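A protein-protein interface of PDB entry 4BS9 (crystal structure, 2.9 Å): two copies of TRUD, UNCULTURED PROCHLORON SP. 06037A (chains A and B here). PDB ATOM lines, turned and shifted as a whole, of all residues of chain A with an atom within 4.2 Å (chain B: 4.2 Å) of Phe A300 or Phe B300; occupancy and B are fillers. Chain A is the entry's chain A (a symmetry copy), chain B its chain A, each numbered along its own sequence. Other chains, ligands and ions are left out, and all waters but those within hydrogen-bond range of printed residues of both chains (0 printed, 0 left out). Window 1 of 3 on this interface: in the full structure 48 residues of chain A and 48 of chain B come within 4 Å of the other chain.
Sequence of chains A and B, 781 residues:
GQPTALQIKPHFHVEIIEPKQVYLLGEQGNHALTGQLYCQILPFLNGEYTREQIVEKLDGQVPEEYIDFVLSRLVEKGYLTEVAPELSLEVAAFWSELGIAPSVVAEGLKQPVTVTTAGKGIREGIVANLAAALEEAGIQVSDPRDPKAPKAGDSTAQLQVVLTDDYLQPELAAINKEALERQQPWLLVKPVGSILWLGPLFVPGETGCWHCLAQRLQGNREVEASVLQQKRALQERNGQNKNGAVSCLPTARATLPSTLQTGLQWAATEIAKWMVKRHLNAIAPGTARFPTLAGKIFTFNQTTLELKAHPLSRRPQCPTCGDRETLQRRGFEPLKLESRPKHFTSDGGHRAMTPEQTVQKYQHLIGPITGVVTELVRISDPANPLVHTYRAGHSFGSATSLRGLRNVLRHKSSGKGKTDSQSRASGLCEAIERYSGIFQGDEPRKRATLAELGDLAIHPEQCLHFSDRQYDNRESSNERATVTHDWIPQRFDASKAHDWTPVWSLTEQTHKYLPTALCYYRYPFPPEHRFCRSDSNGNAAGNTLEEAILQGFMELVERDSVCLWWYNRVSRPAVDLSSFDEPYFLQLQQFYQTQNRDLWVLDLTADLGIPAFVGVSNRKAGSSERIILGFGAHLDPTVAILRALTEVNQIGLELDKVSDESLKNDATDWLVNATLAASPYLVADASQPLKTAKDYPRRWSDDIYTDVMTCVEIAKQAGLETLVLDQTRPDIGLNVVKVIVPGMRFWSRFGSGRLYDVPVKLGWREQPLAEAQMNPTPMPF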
ATOM      1  N   SER A 194      -7.734   8.097  14.045  1.00  0.00           N
ATOM      2  CA  SER A 194      -8.443   7.156  13.188  1.00  0.00           C
ATOM      3  C   SER A 194      -9.681   7.764  12.542  1.00  0.00           C
ATOM      4  O   SER A 194     -10.269   7.149  11.647  1.00  0.00           O
ATOM      5  CB  SER A 194      -8.867   5.938  14.013  1.00  0.00           C
ATOM      6  OG  SER A 194      -9.561   6.347  15.182  1.00  0.00           O
ATOM      7  N   ILE A 195     -10.111   8.933  13.025  1.00  0.00           N
ATOM      8  CA  ILE A 195     -11.209   9.636  12.395  1.00  0.00           C
ATOM      9  C   ILE A 195     -10.827  11.076  12.126  1.00  0.00           C
ATOM     10  O   ILE A 195     -10.415  11.795  13.024  1.00  0.00           O
ATOM     11  CB  ILE A 195     -12.474   9.613  13.242  1.00  0.00           C
ATOM     12  CG1 ILE A 195     -12.751   8.210  13.765  1.00  0.00           C
ATOM     13  CG2 ILE A 195     -13.650  10.107  12.412  1.00  0.00           C
ATOM     14  CD1 ILE A 195     -13.950   8.156  14.689  1.00  0.00           C
ATOM     15  N   LEU A 196     -10.978  11.484  10.874  1.00  0.00           N
ATOM     16  CA  LEU A 196     -10.513  12.778  10.412  1.00  0.00           C
ATOM     17  C   LEU A 196     -11.682  13.726  10.514  1.00  0.00           C
ATOM     18  O   LEU A 196     -12.800  13.355  10.143  1.00  0.00           O
ATOM     19  CB  LEU A 196     -10.057  12.678   8.963  1.00  0.00           C
ATOM     20  CG  LEU A 196      -9.009  11.582   8.730  1.00  0.00           C
ATOM     21  CD1 LEU A 196      -8.857  11.296   7.254  1.00  0.00           C
ATOM     22  CD2 LEU A 196      -7.666  11.969   9.317  1.00  0.00           C
ATOM     23  N   TRP A 266      -7.489  16.313   1.601  1.00  0.00           N
ATOM     24  CA  TRP A 266      -8.904  16.581   1.577  1.00  0.00           C
ATOM     25  C   TRP A 266      -9.198  18.007   2.003  1.00  0.00           C
ATOM     26  O   TRP A 266     -10.038  18.676   1.414  1.00  0.00           O
ATOM     27  CB  TRP A 266      -9.594  15.621   2.517  1.00  0.00           C
ATOM     28  CG  TRP A 266     -11.067  15.721   2.537  1.00  0.00           C
ATOM     29  CD1 TRP A 266     -11.885  16.217   1.557  1.00  0.00           C
ATOM     30  CD2 TRP A 266     -11.926  15.274   3.585  1.00  0.00           C
ATOM     31  NE1 TRP A 266     -13.205  16.120   1.944  1.00  0.00           N
ATOM     32  CE2 TRP A 266     -13.256  15.549   3.187  1.00  0.00           C
ATOM     33  CE3 TRP A 266     -11.699  14.697   4.837  1.00  0.00           C
ATOM     34  CZ2 TRP A 266     -14.345  15.259   3.992  1.00  0.00           C
ATOM     35  CZ3 TRP A 266     -12.779  14.403   5.630  1.00  0.00           C
ATOM     36  CH2 TRP A 266     -14.088  14.683   5.208  1.00  0.00           C
ATOM     37  N   THR A 299     -16.686  14.048   9.432  1.00  0.00           N
ATOM     38  CA  THR A 299     -15.839  13.034  10.003  1.00  0.00           C
ATOM     39  C   THR A 299     -15.705  11.884   9.003  1.00  0.00           C
ATOM     40  O   THR A 299     -16.706  11.398   8.439  1.00  0.00           O
ATOM     41  CB  THR A 299     -16.408  12.487  11.320  1.00  0.00           C
ATOM     42  OG1 THR A 299     -17.689  11.899  11.078  1.00  0.00           O
ATOM     43  CG2 THR A 299     -16.528  13.596  12.363  1.00  0.00           C
ATOM     44  N   PHE A 300     -14.462  11.447   8.806  1.00  0.00           N
ATOM     45  CA  PHE A 300     -14.147  10.366   7.890  1.00  0.00           C
ATOM     46  C   PHE A 300     -13.421   9.286   8.694  1.00  0.00           C
ATOM     47  O   PHE A 300     -12.252   9.449   9.038  1.00  0.00           O
ATOM     48  CB  PHE A 300     -13.273  10.913   6.756  1.00  0.00           C
ATOM     49  CG  PHE A 300     -13.036   9.951   5.622  1.00  0.00           C
ATOM     50  CD1 PHE A 300     -13.603   8.684   5.598  1.00  0.00           C
ATOM     51  CD2 PHE A 300     -12.253  10.350   4.547  1.00  0.00           C
ATOM     52  CE1 PHE A 300     -13.380   7.830   4.542  1.00  0.00           C
ATOM     53  CE2 PHE A 300     -12.039   9.505   3.477  1.00  0.00           C
ATOM     54  CZ  PHE A 300     -12.608   8.239   3.476  1.00  0.00           C
ATOM     55  N   ASN A 301     -14.124   8.202   9.004  1.00  0.00           N
ATOM     56  CA  ASN A 301     -13.585   7.174   9.862  1.00  0.00           C
ATOM     57  C   ASN A 301     -12.715   6.209   9.084  1.00  0.00           C
ATOM     58  O   ASN A 301     -13.156   5.603   8.120  1.00  0.00           O
ATOM     59  CB  ASN A 301     -14.704   6.414  10.525  1.00  0.00           C
ATOM     60  CG  ASN A 301     -14.194   5.475  11.580  1.00  0.00           C
ATOM     61  OD1 ASN A 301     -13.161   4.831  11.395  1.00  0.00           O
ATOM     62  ND2 ASN A 301     -14.899   5.390  12.699  1.00  0.00           N
ATOM     63  N   GLN A 302     -11.477   6.031   9.520  1.00  0.00           N
ATOM     64  CA  GLN A 302     -10.507   5.279   8.732  1.00  0.00           C
ATOM     65  C   GLN A 302     -10.579   3.805   9.004  1.00  0.00           C
ATOM     66  O   GLN A 302     -10.054   3.004   8.245  1.00  0.00           O
ATOM     67  CB  GLN A 302      -9.088   5.787   9.006  1.00  0.00           C
ATOM     68  CG  GLN A 302      -8.903   7.265   8.705  1.00  0.00           C
ATOM     69  CD  GLN A 302      -9.127   7.553   7.242  1.00  0.00           C
ATOM     70  OE1 GLN A 302      -8.238   7.315   6.418  1.00  0.00           O
ATOM     71  NE2 GLN A 302     -10.326   8.030   6.896  1.00  0.00           N
ATOM     72  N   GLU A 306     -16.559   5.369   7.169  1.00  0.00           N
ATOM     73  CA  GLU A 306     -17.835   6.014   7.268  1.00  0.00           C
ATOM     74  C   GLU A 306     -17.627   7.503   7.181  1.00  0.00           C
ATOM     75  O   GLU A 306     -16.764   8.050   7.871  1.00  0.00           O
ATOM     76  CB  GLU A 306     -18.477   5.659   8.587  1.00  0.00           C
ATOM     77  CG  GLU A 306     -19.797   6.380   8.829  1.00  0.00           C
ATOM     78  CD  GLU A 306     -20.427   6.012  10.162  1.00  0.00           C
ATOM     79  OE1 GLU A 306     -19.674   5.560  11.048  1.00  0.00           O
ATOM     80  OE2 GLU A 306     -21.662   6.176  10.329  1.00  0.00           O
ATOM     81  N   LEU A 307     -18.422   8.152   6.332  1.00  0.00           N
ATOM     82  CA  LEU A 307     -18.407   9.609   6.198  1.00  0.00           C
ATOM     83  C   LEU A 307     -19.681  10.227   6.774  1.00  0.00           C
ATOM     84  O   LEU A 307     -20.802   9.843   6.425  1.00  0.00           O
ATOM     85  CB  LEU A 307     -18.255  10.017   4.738  1.00  0.00           C
ATOM     86  CG  LEU A 307     -18.025  11.511   4.522  1.00  0.00           C
ATOM     87  CD1 LEU A 307     -16.647  11.911   5.022  1.00  0.00           C
ATOM     88  CD2 LEU A 307     -18.176  11.873   3.053  1.00  0.00           C
ATOM     89  N   SER B 194     -13.829  13.546 -10.476  1.00  0.00           N
ATOM     90  CA  SER B 194     -14.519  14.153  -9.345  1.00  0.00           C
ATOM     91  C   SER B 194     -15.046  13.124  -8.354  1.00  0.00           C
ATOM     92  O   SER B 194     -15.480  13.495  -7.259  1.00  0.00           O
ATOM     93  CB  SER B 194     -15.694  14.989  -9.857  1.00  0.00           C
ATOM     94  OG  SER B 194     -16.507  14.221 -10.732  1.00  0.00           O
ATOM     95  N   ILE B 195     -15.064  11.849  -8.748  1.00  0.00           N
ATOM     96  CA  ILE B 195     -15.441  10.793  -7.831  1.00  0.00           C
ATOM     97  C   ILE B 195     -14.401   9.692  -7.840  1.00  0.00           C
ATOM     98  O   ILE B 195     -14.068   9.151  -8.883  1.00  0.00           O
ATOM     99  CB  ILE B 195     -16.798  10.191  -8.164  1.00  0.00           C
ATOM    100  CG1 ILE B 195     -17.825  11.283  -8.433  1.00  0.00           C
ATOM    101  CG2 ILE B 195     -17.258   9.306  -7.014  1.00  0.00           C
ATOM    102  CD1 ILE B 195     -19.169  10.730  -8.860  1.00  0.00           C
ATOM    103  N   LEU B 196     -13.902   9.368  -6.656  1.00  0.00           N
ATOM    104  CA  LEU B 196     -12.789   8.451  -6.501  1.00  0.00           C
ATOM    105  C   LEU B 196     -13.378   7.082  -6.261  1.00  0.00           C
ATOM    106  O   LEU B 196     -14.330   6.959  -5.485  1.00  0.00           O
ATOM    107  CB  LEU B 196     -11.938   8.862  -5.308  1.00  0.00           C
ATOM    108  CG  LEU B 196     -11.466  10.320  -5.373  1.00  0.00           C
ATOM    109  CD1 LEU B 196     -10.938  10.769  -4.030  1.00  0.00           C
ATOM    110  CD2 LEU B 196     -10.398  10.509  -6.431  1.00  0.00           C
ATOM    111  N   TRP B 266      -5.603   7.350   0.312  1.00  0.00           N
ATOM    112  CA  TRP B 266      -6.647   6.496   0.817  1.00  0.00           C
ATOM    113  C   TRP B 266      -6.421   5.054   0.404  1.00  0.00           C
ATOM    114  O   TRP B 266      -6.613   4.139   1.196  1.00  0.00           O
ATOM    115  CB  TRP B 266      -7.971   6.975   0.270  1.00  0.00           C
ATOM    116  CG  TRP B 266      -9.152   6.243   0.770  1.00  0.00           C
ATOM    117  CD1 TRP B 266      -9.261   5.525   1.931  1.00  0.00           C
ATOM    118  CD2 TRP B 266     -10.430   6.179   0.139  1.00  0.00           C
ATOM    119  NE1 TRP B 266     -10.533   5.004   2.051  1.00  0.00           N
ATOM    120  CE2 TRP B 266     -11.267   5.387   0.961  1.00  0.00           C
ATOM    121  CE3 TRP B 266     -10.941   6.688  -1.057  1.00  0.00           C
ATOM    122  CZ2 TRP B 266     -12.581   5.104   0.626  1.00  0.00           C
ATOM    123  CZ3 TRP B 266     -12.245   6.414  -1.384  1.00  0.00           C
ATOM    124  CH2 TRP B 266     -13.053   5.629  -0.547  1.00  0.00           C
ATOM    125  N   THR B 299     -16.985   4.706  -3.494  1.00  0.00           N
ATOM    126  CA  THR B 299     -16.931   5.935  -4.241  1.00  0.00           C
ATOM    127  C   THR B 299     -16.965   7.110  -3.261  1.00  0.00           C
ATOM    128  O   THR B 299     -17.802   7.157  -2.337  1.00  0.00           O
ATOM    129  CB  THR B 299     -18.110   6.065  -5.217  1.00  0.00           C
ATOM    130  OG1 THR B 299     -19.339   6.055  -4.485  1.00  0.00           O
ATOM    131  CG2 THR B 299     -18.099   4.931  -6.238  1.00  0.00           C
ATOM    132  N   PHE B 300     -16.058   8.059  -3.485  1.00  0.00           N
ATOM    133  CA  PHE B 300     -15.941   9.242  -2.654  1.00  0.00           C
ATOM    134  C   PHE B 300     -16.098  10.458  -3.569  1.00  0.00           C
ATOM    135  O   PHE B 300     -15.185  10.793  -4.319  1.00  0.00           O
ATOM    136  CB  PHE B 300     -14.575   9.230  -1.957  1.00  0.00           C
ATOM    137  CG  PHE B 300     -14.394  10.292  -0.905  1.00  0.00           C
ATOM    138  CD1 PHE B 300     -15.406  11.182  -0.572  1.00  0.00           C
ATOM    139  CD2 PHE B 300     -13.189  10.367  -0.219  1.00  0.00           C
ATOM    140  CE1 PHE B 300     -15.216  12.134   0.403  1.00  0.00           C
ATOM    141  CE2 PHE B 300     -12.998  11.309   0.772  1.00  0.00           C
ATOM    142  CZ  PHE B 300     -14.019  12.195   1.084  1.00  0.00           C
ATOM    143  N   ASN B 301     -17.262  11.098  -3.513  1.00  0.00           N
ATOM    144  CA  ASN B 301     -17.572  12.180  -4.416  1.00  0.00           C
ATOM    145  C   ASN B 301     -16.995  13.490  -3.920  1.00  0.00           C
ATOM    146  O   ASN B 301     -17.279  13.923  -2.815  1.00  0.00           O
ATOM    147  CB  ASN B 301     -19.064  12.317  -4.569  1.00  0.00           C
ATOM    148  CG  ASN B 301     -19.428  13.291  -5.651  1.00  0.00           C
ATOM    149  OD1 ASN B 301     -18.789  14.334  -5.794  1.00  0.00           O
ATOM    150  ND2 ASN B 301     -20.447  12.964  -6.434  1.00  0.00           N
ATOM    151  N   GLN B 302     -16.205  14.152  -4.754  1.00  0.00           N
ATOM    152  CA  GLN B 302     -15.450  15.316  -4.303  1.00  0.00           C
ATOM    153  C   GLN B 302     -16.249  16.581  -4.404  1.00  0.00           C
ATOM    154  O   GLN B 302     -15.893  17.592  -3.818  1.00  0.00           O
ATOM    155  CB  GLN B 302     -14.154  15.455  -5.108  1.00  0.00           C
ATOM    156  CG  GLN B 302     -13.250  14.238  -5.019  1.00  0.00           C
ATOM    157  CD  GLN B 302     -12.787  14.007  -3.603  1.00  0.00           C
ATOM    158  OE1 GLN B 302     -11.863  14.677  -3.135  1.00  0.00           O
ATOM    159  NE2 GLN B 302     -13.446  13.085  -2.895  1.00  0.00           N
ATOM    160  N   GLU B 306     -19.853  12.731  -0.696  1.00  0.00           N
ATOM    161  CA  GLU B 306     -20.662  11.589  -0.387  1.00  0.00           C
ATOM    162  C   GLU B 306     -19.810  10.354  -0.507  1.00  0.00           C
ATOM    163  O   GLU B 306     -19.105  10.180  -1.504  1.00  0.00           O
ATOM    164  CB  GLU B 306     -21.818  11.515  -1.354  1.00  0.00           C
ATOM    165  CG  GLU B 306     -22.681  10.274  -1.169  1.00  0.00           C
ATOM    166  CD  GLU B 306     -23.838  10.215  -2.153  1.00  0.00           C
ATOM    167  OE1 GLU B 306     -23.729  10.874  -3.206  1.00  0.00           O
ATOM    168  OE2 GLU B 306     -24.847   9.516  -1.881  1.00  0.00           O
ATOM    169  N   LEU B 307     -19.881   9.497   0.511  1.00  0.00           N
ATOM    170  CA  LEU B 307     -19.186   8.210   0.507  1.00  0.00           C
ATOM    171  C   LEU B 307     -20.175   7.053   0.374  1.00  0.00           C
ATOM    172  O   LEU B 307     -21.144   6.937   1.130  1.00  0.00           O
ATOM    173  CB  LEU B 307     -18.362   8.035   1.776  1.00  0.00           C
ATOM    174  CG  LEU B 307     -17.443   6.815   1.767  1.00  0.00           C
ATOM    175  CD1 LEU B 307     -16.310   7.015   0.777  1.00  0.00           C
ATOM    176  CD2 LEU B 307     -16.885   6.550   3.158  1.00  0.00           C
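N of Phe B300 is in hydrogen-bond range of O of Leu B196, at 2.9 Å. The backbone carbonyl oxygen (O) of Phe B300 sits at hydrogen-bond distance from the side-chain amide nitrogen (NE2) of Gln B302. O of Leu A196 is in hydrogen-bond range of N of Phe A300, 2.9 Å away. The backbone carbonyl oxygen (O) of Phe A300 sits at hydrogen-bond distance from the side-chain amide nitrogen (NE2) of Gln A302, at 3.2 Å.
Printed residues of chain B within 4 Å of Phe A300: Phe B300 (3.4 Å) and Leu B307 (3.98 Å). Of the printed residues of chain A, Phe B300 touches Phe A300 (3.4 Å) and Leu A307 (3.98 Å). Of the printed residues of chain A, Leu B307 touches Phe A300 (3.98 Å) and Leu A307 (3.6 Å). Printed residues of chain B within 4 Å of Leu A307: Phe B300 (3.98 Å) and Leu B307 (3.6 Å). The nearest printed residue of chain A that does not touch Phe B300 is Trp A266 (4.03 Å).
Among the printed residues, merely in contact across the chains: Phe A300 with Phe B300 (3.4 Å), Leu A307 with Leu B307 (3.6 Å), Phe A300 with Leu B307 (3.98 Å) and Leu A307 with Phe B300 (3.98 Å).
Of the 10 printed residues of chain B, 2 touch a printed residue of chain A. Hydrophobic or aromatic side chains of chain B that line the printed part of chain A: Phe B300 and Leu B307. Printed residues of chain A that touch a printed residue of chain B: Phe A300 and Leu A307. Hydrophobic or aromatic side chains of chain A that line the printed part of chain B: Phe A300 and Leu A307. Among the printed residues, 4 pairs touch across the chains. Among the printed residues, no Asp or Glu carboxylate lies within 4 Å of a Lys or Arg side-chain nitrogen of the other chain.
Phe A300 touches its own counterpart, Phe B300. Phe A300 touches Leu B307, and with the chains exchanged Leu A307 touches Phe B300. Leu B307 touches its own counterpart, Leu A307. Positions printed for both chains: 194, 195, 196, 266, 299, 300, 301, 302, 306 and 307. Of the 4 pairs that touch across the chains among the printed residues, 4 have their exchanged pair printed and touching as well.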
